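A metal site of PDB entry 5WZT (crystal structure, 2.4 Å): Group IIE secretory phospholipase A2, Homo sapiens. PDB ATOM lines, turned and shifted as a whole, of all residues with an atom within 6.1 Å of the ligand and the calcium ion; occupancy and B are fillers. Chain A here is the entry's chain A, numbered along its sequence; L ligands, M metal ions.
A ring nitrogen (ND1) of His 46 lies within hydrogen-bond range of an oxygen (O4) of the ligand (3.1 Å). An oxygen (O5) of the ligand sits close to the backbone NH (N) of Gly 28 (2.8 Å). The backbone carbonyl oxygen (O) of Cys 43 is in hydrogen-bond range of a nitrogen (N1) of the ligand (2.9 Å).
The side-chain sulfur of Cys 43 is disulfide-bonded to the side-chain sulfur of Cys 27 (2.0 Å). N of Phe 97 lies within hydrogen-bond range of SG of Cys 42. The backbone carbonyl oxygen of Cys 27 sits at hydrogen-bond distance from the backbone NH of Asp 22, 3.0 Å away.
The calcium ion is bound by O of Tyr 26, O of Gly 28, O5 of the ligand, O of Gly 30 and OD1 of Asp 47. Slightly farther from the calcium ion lies OD2 of Asp 47 (3.0 Å).
Four residues have an atom within 4 Å of the calcium ion: Tyr 26, Gly 28, Gly 30 and Asp 47. The nearest printed residue that does not touch the calcium ion is Ile 29 (4.2 Å).
Residues that only touch the ligand: Leu 2 (3.5 Å), Phe 5 (3.2 Å), Gly 6 (3.5 Å), Ile 9 (3.7 Å), Ala 17 (3.5 Å), Leu 18 (3.8 Å), Tyr 20 (3.4 Å), Asn 21 (3.6 Å), Cys 27 (3.3 Å), Ile 29 (3.5 Å), Tyr 50 (3.9 Å), Lys 61 (3.5 Å) and Phe 97 (3.6 Å). Hydrophobic or aromatic side chains within 4 Å of the ligand: Leu 2, Phe 5, Ile 9, Ala 17, Leu 18, Tyr 20, Ile 29, His 46, Tyr 50 and Phe 97. Of the 27 residues printed, 19 come within 4 Å of the ligand. The nearest printed residue that does not touch the ligand is His 44 (4.8 Å).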
ATOM      1  N   LEU A   2     -26.376   4.896   7.184  1.00  0.00           N
ATOM      2  CA  LEU A   2     -25.275   4.583   8.111  1.00  0.00           C
ATOM      3  C   LEU A   2     -25.030   5.610   9.223  1.00  0.00           C
ATOM      4  O   LEU A   2     -24.060   5.466   9.992  1.00  0.00           O
ATOM      5  CB  LEU A   2     -23.973   4.371   7.308  1.00  0.00           C
ATOM      6  CG  LEU A   2     -23.833   3.083   6.495  1.00  0.00           C
ATOM      7  CD1 LEU A   2     -22.592   3.135   5.612  1.00  0.00           C
ATOM      8  CD2 LEU A   2     -23.789   1.848   7.406  1.00  0.00           C
ATOM      9  N   VAL A   3     -25.888   6.617   9.347  1.00  0.00           N
ATOM     10  CA  VAL A   3     -25.644   7.740  10.276  1.00  0.00           C
ATOM     11  C   VAL A   3     -25.558   7.306  11.763  1.00  0.00           C
ATOM     12  O   VAL A   3     -24.535   7.534  12.404  1.00  0.00           O
ATOM     13  CB  VAL A   3     -26.636   8.925  10.052  1.00  0.00           C
ATOM     14  CG1 VAL A   3     -28.096   8.554  10.347  1.00  0.00           C
ATOM     15  CG2 VAL A   3     -26.218  10.161  10.856  1.00  0.00           C
ATOM     16  N   PHE A   5     -25.236   4.335  13.213  1.00  0.00           N
ATOM     17  CA  PHE A   5     -24.146   3.389  13.466  1.00  0.00           C
ATOM     18  C   PHE A   5     -22.777   4.078  13.583  1.00  0.00           C
ATOM     19  O   PHE A   5     -22.033   3.865  14.547  1.00  0.00           O
ATOM     20  CB  PHE A   5     -24.129   2.325  12.368  1.00  0.00           C
ATOM     21  CG  PHE A   5     -23.177   1.186  12.616  1.00  0.00           C
ATOM     22  CD1 PHE A   5     -22.918   0.690  13.905  1.00  0.00           C
ATOM     23  CD2 PHE A   5     -22.553   0.572  11.538  1.00  0.00           C
ATOM     24  CE1 PHE A   5     -22.031  -0.364  14.097  1.00  0.00           C
ATOM     25  CE2 PHE A   5     -21.666  -0.483  11.729  1.00  0.00           C
ATOM     26  CZ  PHE A   5     -21.412  -0.954  13.005  1.00  0.00           C
ATOM     27  N   GLY A   6     -22.487   4.928  12.582  1.00  0.00           N
ATOM     28  CA  GLY A   6     -21.302   5.756  12.584  1.00  0.00           C
ATOM     29  C   GLY A   6     -21.204   6.597  13.827  1.00  0.00           C
ATOM     30  O   GLY A   6     -20.112   6.731  14.402  1.00  0.00           O
ATOM     31  N   VAL A   7     -22.344   7.143  14.285  1.00  0.00           N
ATOM     32  CA  VAL A   7     -22.325   7.896  15.538  1.00  0.00           C
ATOM     33  C   VAL A   7     -21.976   6.975  16.710  1.00  0.00           C
ATOM     34  O   VAL A   7     -21.133   7.310  17.545  1.00  0.00           O
ATOM     35  CB  VAL A   7     -23.649   8.654  15.816  1.00  0.00           C
ATOM     36  CG1 VAL A   7     -23.648   9.301  17.213  1.00  0.00           C
ATOM     37  CG2 VAL A   7     -23.879   9.731  14.766  1.00  0.00           C
ATOM     38  N   ILE A   9     -20.333   4.185  16.663  1.00  0.00           N
ATOM     39  CA  ILE A   9     -18.913   3.827  16.551  1.00  0.00           C
ATOM     40  C   ILE A   9     -18.009   4.918  17.139  1.00  0.00           C
ATOM     41  O   ILE A   9     -17.087   4.610  17.902  1.00  0.00           O
ATOM     42  CB  ILE A   9     -18.504   3.486  15.109  1.00  0.00           C
ATOM     43  CG1 ILE A   9     -19.213   2.203  14.654  1.00  0.00           C
ATOM     44  CG2 ILE A   9     -16.994   3.268  15.014  1.00  0.00           C
ATOM     45  CD1 ILE A   9     -19.386   2.105  13.158  1.00  0.00           C
ATOM     46  N   ALA A  17     -15.961   6.845  12.247  1.00  0.00           N
ATOM     47  CA  ALA A  17     -16.479   5.636  11.607  1.00  0.00           C
ATOM     48  C   ALA A  17     -15.755   5.265  10.300  1.00  0.00           C
ATOM     49  O   ALA A  17     -15.675   4.084   9.938  1.00  0.00           O
ATOM     50  CB  ALA A  17     -17.959   5.793  11.331  1.00  0.00           C
ATOM     51  N   LEU A  18     -15.238   6.272   9.598  1.00  0.00           N
ATOM     52  CA  LEU A  18     -14.438   6.071   8.383  1.00  0.00           C
ATOM     53  C   LEU A  18     -13.221   5.163   8.605  1.00  0.00           C
ATOM     54  O   LEU A  18     -12.787   4.478   7.675  1.00  0.00           O
ATOM     55  CB  LEU A  18     -13.960   7.416   7.811  1.00  0.00           C
ATOM     56  CG  LEU A  18     -15.007   8.474   7.431  1.00  0.00           C
ATOM     57  CD1 LEU A  18     -14.293   9.688   6.849  1.00  0.00           C
ATOM     58  CD2 LEU A  18     -16.040   7.917   6.461  1.00  0.00           C
ATOM     59  N   TYR A  20     -13.207   2.502  10.279  1.00  0.00           N
ATOM     60  CA  TYR A  20     -13.725   1.141  10.179  1.00  0.00           C
ATOM     61  C   TYR A  20     -14.404   0.865   8.835  1.00  0.00           C
ATOM     62  O   TYR A  20     -15.070  -0.146   8.682  1.00  0.00           O
ATOM     63  CB  TYR A  20     -14.703   0.874  11.331  1.00  0.00           C
ATOM     64  CG  TYR A  20     -14.045   0.881  12.694  1.00  0.00           C
ATOM     65  CD1 TYR A  20     -13.799   2.077  13.384  1.00  0.00           C
ATOM     66  CD2 TYR A  20     -13.671  -0.322  13.298  1.00  0.00           C
ATOM     67  CE1 TYR A  20     -13.201   2.071  14.631  1.00  0.00           C
ATOM     68  CE2 TYR A  20     -13.059  -0.326  14.543  1.00  0.00           C
ATOM     69  CZ  TYR A  20     -12.824   0.860  15.205  1.00  0.00           C
ATOM     70  OH  TYR A  20     -12.233   0.837  16.439  1.00  0.00           O
ATOM     71  N   ASN A  21     -14.236   1.742   7.861  1.00  0.00           N
ATOM     72  CA  ASN A  21     -14.808   1.527   6.520  1.00  0.00           C
ATOM     73  C   ASN A  21     -13.672   0.975   5.671  1.00  0.00           C
ATOM     74  O   ASN A  21     -12.520   1.450   5.766  1.00  0.00           O
ATOM     75  CB  ASN A  21     -15.380   2.845   5.968  1.00  0.00           C
ATOM     76  CG  ASN A  21     -16.130   2.680   4.645  1.00  0.00           C
ATOM     77  OD1 ASN A  21     -15.859   3.421   3.696  1.00  0.00           O
ATOM     78  ND2 ASN A  21     -17.077   1.733   4.567  1.00  0.00           N
ATOM     79  N   ASP A  22     -13.985  -0.082   4.917  1.00  0.00           N
ATOM     80  CA  ASP A  22     -13.000  -0.895   4.185  1.00  0.00           C
ATOM     81  C   ASP A  22     -11.908  -1.486   5.066  1.00  0.00           C
ATOM     82  O   ASP A  22     -10.898  -1.961   4.541  1.00  0.00           O
ATOM     83  CB  ASP A  22     -12.370  -0.106   3.033  1.00  0.00           C
ATOM     84  CG  ASP A  22     -13.380   0.450   2.086  1.00  0.00           C
ATOM     85  OD1 ASP A  22     -14.475  -0.142   1.962  1.00  0.00           O
ATOM     86  OD2 ASP A  22     -13.085   1.492   1.482  1.00  0.00           O
ATOM     87  N   CYS A  25     -11.004  -7.354   5.749  1.00  0.00           N
ATOM     88  CA  CYS A  25     -11.739  -8.091   4.745  1.00  0.00           C
ATOM     89  C   CYS A  25     -13.244  -8.041   4.892  1.00  0.00           C
ATOM     90  O   CYS A  25     -13.941  -8.377   3.920  1.00  0.00           O
ATOM     91  CB  CYS A  25     -11.212  -9.528   4.721  1.00  0.00           C
ATOM     92  SG  CYS A  25      -9.511  -9.611   4.093  1.00  0.00           S
ATOM     93  N   TYR A  26     -13.753  -7.578   6.049  1.00  0.00           N
ATOM     94  CA  TYR A  26     -15.192  -7.570   6.343  1.00  0.00           C
ATOM     95  C   TYR A  26     -15.882  -6.233   6.657  1.00  0.00           C
ATOM     96  O   TYR A  26     -17.092  -6.146   6.507  1.00  0.00           O
ATOM     97  CB  TYR A  26     -15.525  -8.606   7.444  1.00  0.00           C
ATOM     98  CG  TYR A  26     -15.544  -9.998   6.899  1.00  0.00           C
ATOM     99  CD1 TYR A  26     -16.707 -10.541   6.347  1.00  0.00           C
ATOM    100  CD2 TYR A  26     -14.379 -10.759   6.842  1.00  0.00           C
ATOM    101  CE1 TYR A  26     -16.716 -11.819   5.792  1.00  0.00           C
ATOM    102  CE2 TYR A  26     -14.374 -12.030   6.294  1.00  0.00           C
ATOM    103  CZ  TYR A  26     -15.544 -12.554   5.766  1.00  0.00           C
ATOM    104  OH  TYR A  26     -15.550 -13.807   5.209  1.00  0.00           O
ATOM    105  N   CYS A  27     -15.158  -5.214   7.092  1.00  0.00           N
ATOM    106  CA  CYS A  27     -15.818  -3.961   7.464  1.00  0.00           C
ATOM    107  C   CYS A  27     -16.032  -3.111   6.209  1.00  0.00           C
ATOM    108  O   CYS A  27     -15.066  -2.781   5.497  1.00  0.00           O
ATOM    109  CB  CYS A  27     -15.012  -3.194   8.491  1.00  0.00           C
ATOM    110  SG  CYS A  27     -14.466  -4.156   9.904  1.00  0.00           S
ATOM    111  N   GLY A  28     -17.292  -2.752   5.961  1.00  0.00           N
ATOM    112  CA  GLY A  28     -17.705  -2.117   4.705  1.00  0.00           C
ATOM    113  C   GLY A  28     -18.615  -3.077   3.983  1.00  0.00           C
ATOM    114  O   GLY A  28     -18.805  -4.184   4.455  1.00  0.00           O
ATOM    115  N   ILE A  29     -19.184  -2.669   2.848  1.00  0.00           N
ATOM    116  CA  ILE A  29     -20.184  -3.521   2.208  1.00  0.00           C
ATOM    117  C   ILE A  29     -19.604  -4.878   1.775  1.00  0.00           C
ATOM    118  O   ILE A  29     -18.450  -4.968   1.340  1.00  0.00           O
ATOM    119  CB  ILE A  29     -20.941  -2.824   1.034  1.00  0.00           C
ATOM    120  CG1 ILE A  29     -19.987  -2.391  -0.108  1.00  0.00           C
ATOM    121  CG2 ILE A  29     -21.785  -1.661   1.576  1.00  0.00           C
ATOM    122  CD1 ILE A  29     -20.215  -3.155  -1.409  1.00  0.00           C
ATOM    123  N   GLY A  30     -20.404  -5.934   1.969  1.00  0.00           N
ATOM    124  CA  GLY A  30     -19.996  -7.294   1.677  1.00  0.00           C
ATOM    125  C   GLY A  30     -18.884  -7.802   2.578  1.00  0.00           C
ATOM    126  O   GLY A  30     -18.797  -7.436   3.749  1.00  0.00           O
ATOM    127  N   GLY A  31     -18.020  -8.634   2.027  1.00  0.00           N
ATOM    128  CA  GLY A  31     -16.927  -9.222   2.779  1.00  0.00           C
ATOM    129  C   GLY A  31     -16.807 -10.687   2.440  1.00  0.00           C
ATOM    130  O   GLY A  31     -17.794 -11.323   2.091  1.00  0.00           O
ATOM    131  N   CYS A  42     -15.361  -8.663  14.419  1.00  0.00           N
ATOM    132  CA  CYS A  42     -16.535  -7.894  14.831  1.00  0.00           C
ATOM    133  C   CYS A  42     -17.428  -7.658  13.633  1.00  0.00           C
ATOM    134  O   CYS A  42     -18.633  -7.873  13.727  1.00  0.00           O
ATOM    135  CB  CYS A  42     -16.187  -6.537  15.454  1.00  0.00           C
ATOM    136  SG  CYS A  42     -14.992  -6.554  16.806  1.00  0.00           S
ATOM    137  N   CYS A  43     -16.828  -7.242  12.525  1.00  0.00           N
ATOM    138  CA  CYS A  43     -17.554  -6.971  11.272  1.00  0.00           C
ATOM    139  C   CYS A  43     -18.143  -8.206  10.618  1.00  0.00           C
ATOM    140  O   CYS A  43     -19.251  -8.141  10.090  1.00  0.00           O
ATOM    141  CB  CYS A  43     -16.661  -6.238  10.261  1.00  0.00           C
ATOM    142  SG  CYS A  43     -16.201  -4.610  10.847  1.00  0.00           S
ATOM    143  N   HIS A  44     -17.400  -9.324  10.625  1.00  0.00           N
ATOM    144  CA  HIS A  44     -17.940 -10.630  10.205  1.00  0.00           C
ATOM    145  C   HIS A  44     -19.166 -11.016  11.049  1.00  0.00           C
ATOM    146  O   HIS A  44     -20.220 -11.375  10.497  1.00  0.00           O
ATOM    147  CB  HIS A  44     -16.855 -11.722  10.288  1.00  0.00           C
ATOM    148  CG  HIS A  44     -17.349 -13.115  10.032  1.00  0.00           C
ATOM    149  ND1 HIS A  44     -17.920 -13.901  11.016  1.00  0.00           N
ATOM    150  CD2 HIS A  44     -17.317 -13.881   8.911  1.00  0.00           C
ATOM    151  CE1 HIS A  44     -18.244 -15.068  10.500  1.00  0.00           C
ATOM    152  NE2 HIS A  44     -17.893 -15.089   9.225  1.00  0.00           N
ATOM    153  N   HIS A  46     -21.010  -8.888  12.700  1.00  0.00           N
ATOM    154  CA  HIS A  46     -22.027  -7.872  12.378  1.00  0.00           C
ATOM    155  C   HIS A  46     -22.766  -8.190  11.073  1.00  0.00           C
ATOM    156  O   HIS A  46     -23.995  -8.142  11.039  1.00  0.00           O
ATOM    157  CB  HIS A  46     -21.393  -6.486  12.327  1.00  0.00           C
ATOM    158  CG  HIS A  46     -22.386  -5.382  12.195  1.00  0.00           C
ATOM    159  ND1 HIS A  46     -22.722  -4.818  10.987  1.00  0.00           N
ATOM    160  CD2 HIS A  46     -23.127  -4.732  13.121  1.00  0.00           C
ATOM    161  CE1 HIS A  46     -23.620  -3.870  11.171  1.00  0.00           C
ATOM    162  NE2 HIS A  46     -23.893  -3.811  12.466  1.00  0.00           N
ATOM    163  N   ASP A  47     -22.034  -8.534  10.017  1.00  0.00           N
ATOM    164  CA  ASP A  47     -22.623  -9.092   8.783  1.00  0.00           C
ATOM    165  C   ASP A  47     -23.593 -10.273   9.063  1.00  0.00           C
ATOM    166  O   ASP A  47     -24.718 -10.339   8.531  1.00  0.00           O
ATOM    167  CB  ASP A  47     -21.533  -9.617   7.853  1.00  0.00           C
ATOM    168  CG  ASP A  47     -20.747  -8.517   7.111  1.00  0.00           C
ATOM    169  OD1 ASP A  47     -20.970  -7.306   7.280  1.00  0.00           O
ATOM    170  OD2 ASP A  47     -19.888  -8.912   6.307  1.00  0.00           O
ATOM    171  N   TYR A  50     -26.766  -8.980  10.702  1.00  0.00           N
ATOM    172  CA  TYR A  50     -27.664  -8.425   9.689  1.00  0.00           C
ATOM    173  C   TYR A  50     -28.370  -9.525   8.883  1.00  0.00           C
ATOM    174  O   TYR A  50     -29.567  -9.438   8.639  1.00  0.00           O
ATOM    175  CB  TYR A  50     -26.943  -7.378   8.809  1.00  0.00           C
ATOM    176  CG  TYR A  50     -26.936  -5.942   9.365  1.00  0.00           C
ATOM    177  CD1 TYR A  50     -27.065  -5.672  10.723  1.00  0.00           C
ATOM    178  CD2 TYR A  50     -26.757  -4.830   8.509  1.00  0.00           C
ATOM    179  CE1 TYR A  50     -27.060  -4.352  11.207  1.00  0.00           C
ATOM    180  CE2 TYR A  50     -26.730  -3.518   8.984  1.00  0.00           C
ATOM    181  CZ  TYR A  50     -26.871  -3.272  10.334  1.00  0.00           C
ATOM    182  OH  TYR A  50     -26.876  -1.966  10.826  1.00  0.00           O
ATOM    183  N   LYS A  61     -30.102  -2.673   6.945  1.00  0.00           N
ATOM    184  CA  LYS A  61     -29.374  -1.638   6.188  1.00  0.00           C
ATOM    185  C   LYS A  61     -30.072  -0.301   6.224  1.00  0.00           C
ATOM    186  O   LYS A  61     -29.421   0.720   6.107  1.00  0.00           O
ATOM    187  CB  LYS A  61     -29.165  -2.063   4.728  1.00  0.00           C
ATOM    188  CG  LYS A  61     -27.949  -2.956   4.548  1.00  0.00           C
ATOM    189  CD  LYS A  61     -28.064  -3.886   3.347  1.00  0.00           C
ATOM    190  CE  LYS A  61     -26.741  -4.615   3.133  1.00  0.00           C
ATOM    191  NZ  LYS A  61     -26.974  -5.983   2.588  1.00  0.00           N
ATOM    192  N   ALA A  93     -21.454  -4.742  17.795  1.00  0.00           N
ATOM    193  CA  ALA A  93     -20.319  -4.397  16.935  1.00  0.00           C
ATOM    194  C   ALA A  93     -19.468  -3.233  17.485  1.00  0.00           C
ATOM    195  O   ALA A  93     -18.238  -3.277  17.435  1.00  0.00           O
ATOM    196  CB  ALA A  93     -20.801  -4.093  15.518  1.00  0.00           C
ATOM    197  N   PHE A  97     -15.714  -3.352  18.703  1.00  0.00           N
ATOM    198  CA  PHE A  97     -14.656  -2.436  18.224  1.00  0.00           C
ATOM    199  C   PHE A  97     -13.886  -1.775  19.373  1.00  0.00           C
ATOM    200  O   PHE A  97     -12.659  -1.802  19.372  1.00  0.00           O
ATOM    201  CB  PHE A  97     -15.188  -1.311  17.329  1.00  0.00           C
ATOM    202  CG  PHE A  97     -15.790  -1.758  16.032  1.00  0.00           C
ATOM    203  CD1 PHE A  97     -15.257  -2.831  15.297  1.00  0.00           C
ATOM    204  CD2 PHE A  97     -16.848  -1.035  15.489  1.00  0.00           C
ATOM    205  CE1 PHE A  97     -15.817  -3.192  14.075  1.00  0.00           C
ATOM    206  CE2 PHE A  97     -17.405  -1.376  14.255  1.00  0.00           C
ATOM    207  CZ  PHE A  97     -16.875  -2.464  13.541  1.00  0.00           C
HETATM  208  O1  LIG L   1     -22.192  -4.838   4.796  1.00  0.00           O
HETATM  209  C1  LIG L   1     -23.159  -4.588   5.553  1.00  0.00           C
HETATM  210  O2  LIG L   1     -24.259  -5.181   5.535  1.00  0.00           O
HETATM  211  C2  LIG L   1     -22.973  -3.490   6.640  1.00  0.00           C
HETATM  212  O3  LIG L   1     -21.567  -3.211   6.912  1.00  0.00           O
HETATM  213  C3  LIG L   1     -21.044  -1.955   6.677  1.00  0.00           C
HETATM  214  C4  LIG L   1     -21.394  -1.256   5.508  1.00  0.00           C
HETATM  215  C5  LIG L   1     -20.859  -0.017   5.283  1.00  0.00           C
HETATM  216  C6  LIG L   1     -19.969   0.490   6.223  1.00  0.00           C
HETATM  217  C7  LIG L   1     -19.652  -0.195   7.329  1.00  0.00           C
HETATM  218  C8  LIG L   1     -20.171  -1.417   7.578  1.00  0.00           C
HETATM  219  C9  LIG L   1     -19.611  -1.819   8.757  1.00  0.00           C
HETATM  220  C10 LIG L   1     -19.813  -2.983   9.414  1.00  0.00           C
HETATM  221  O4  LIG L   1     -20.186  -3.071  10.580  1.00  0.00           O
HETATM  222  C11 LIG L   1     -19.493  -4.264   8.653  1.00  0.00           C
HETATM  223  O5  LIG L   1     -19.070  -4.243   7.509  1.00  0.00           O
HETATM  224  N1  LIG L   1     -19.797  -5.374   9.273  1.00  0.00           N
HETATM  225  C12 LIG L   1     -18.804  -0.860   9.198  1.00  0.00           C
HETATM  226  C13 LIG L   1     -18.006  -0.927  10.501  1.00  0.00           C
HETATM  227  N2  LIG L   1     -18.814   0.146   8.324  1.00  0.00           N
HETATM  228  C14 LIG L   1     -18.068   1.489   8.383  1.00  0.00           C
HETATM  229  C15 LIG L   1     -18.964   2.559   8.693  1.00  0.00           C
HETATM  230  C16 LIG L   1     -18.779   3.839   8.132  1.00  0.00           C
HETATM  231  C17 LIG L   1     -19.658   4.894   8.439  1.00  0.00           C
HETATM  232 BR1  LIG L   1     -19.434   6.643   7.707  1.00  0.00          BR
HETATM  233  C18 LIG L   1     -20.737   4.675   9.279  1.00  0.00           C
HETATM  234  C19 LIG L   1     -20.942   3.417   9.828  1.00  0.00           C
HETATM  235  C20 LIG L   1     -20.066   2.365   9.544  1.00  0.00           C
HETATM  236 CA    CA M   1     -19.218  -6.012   5.791  1.00  0.00          CA
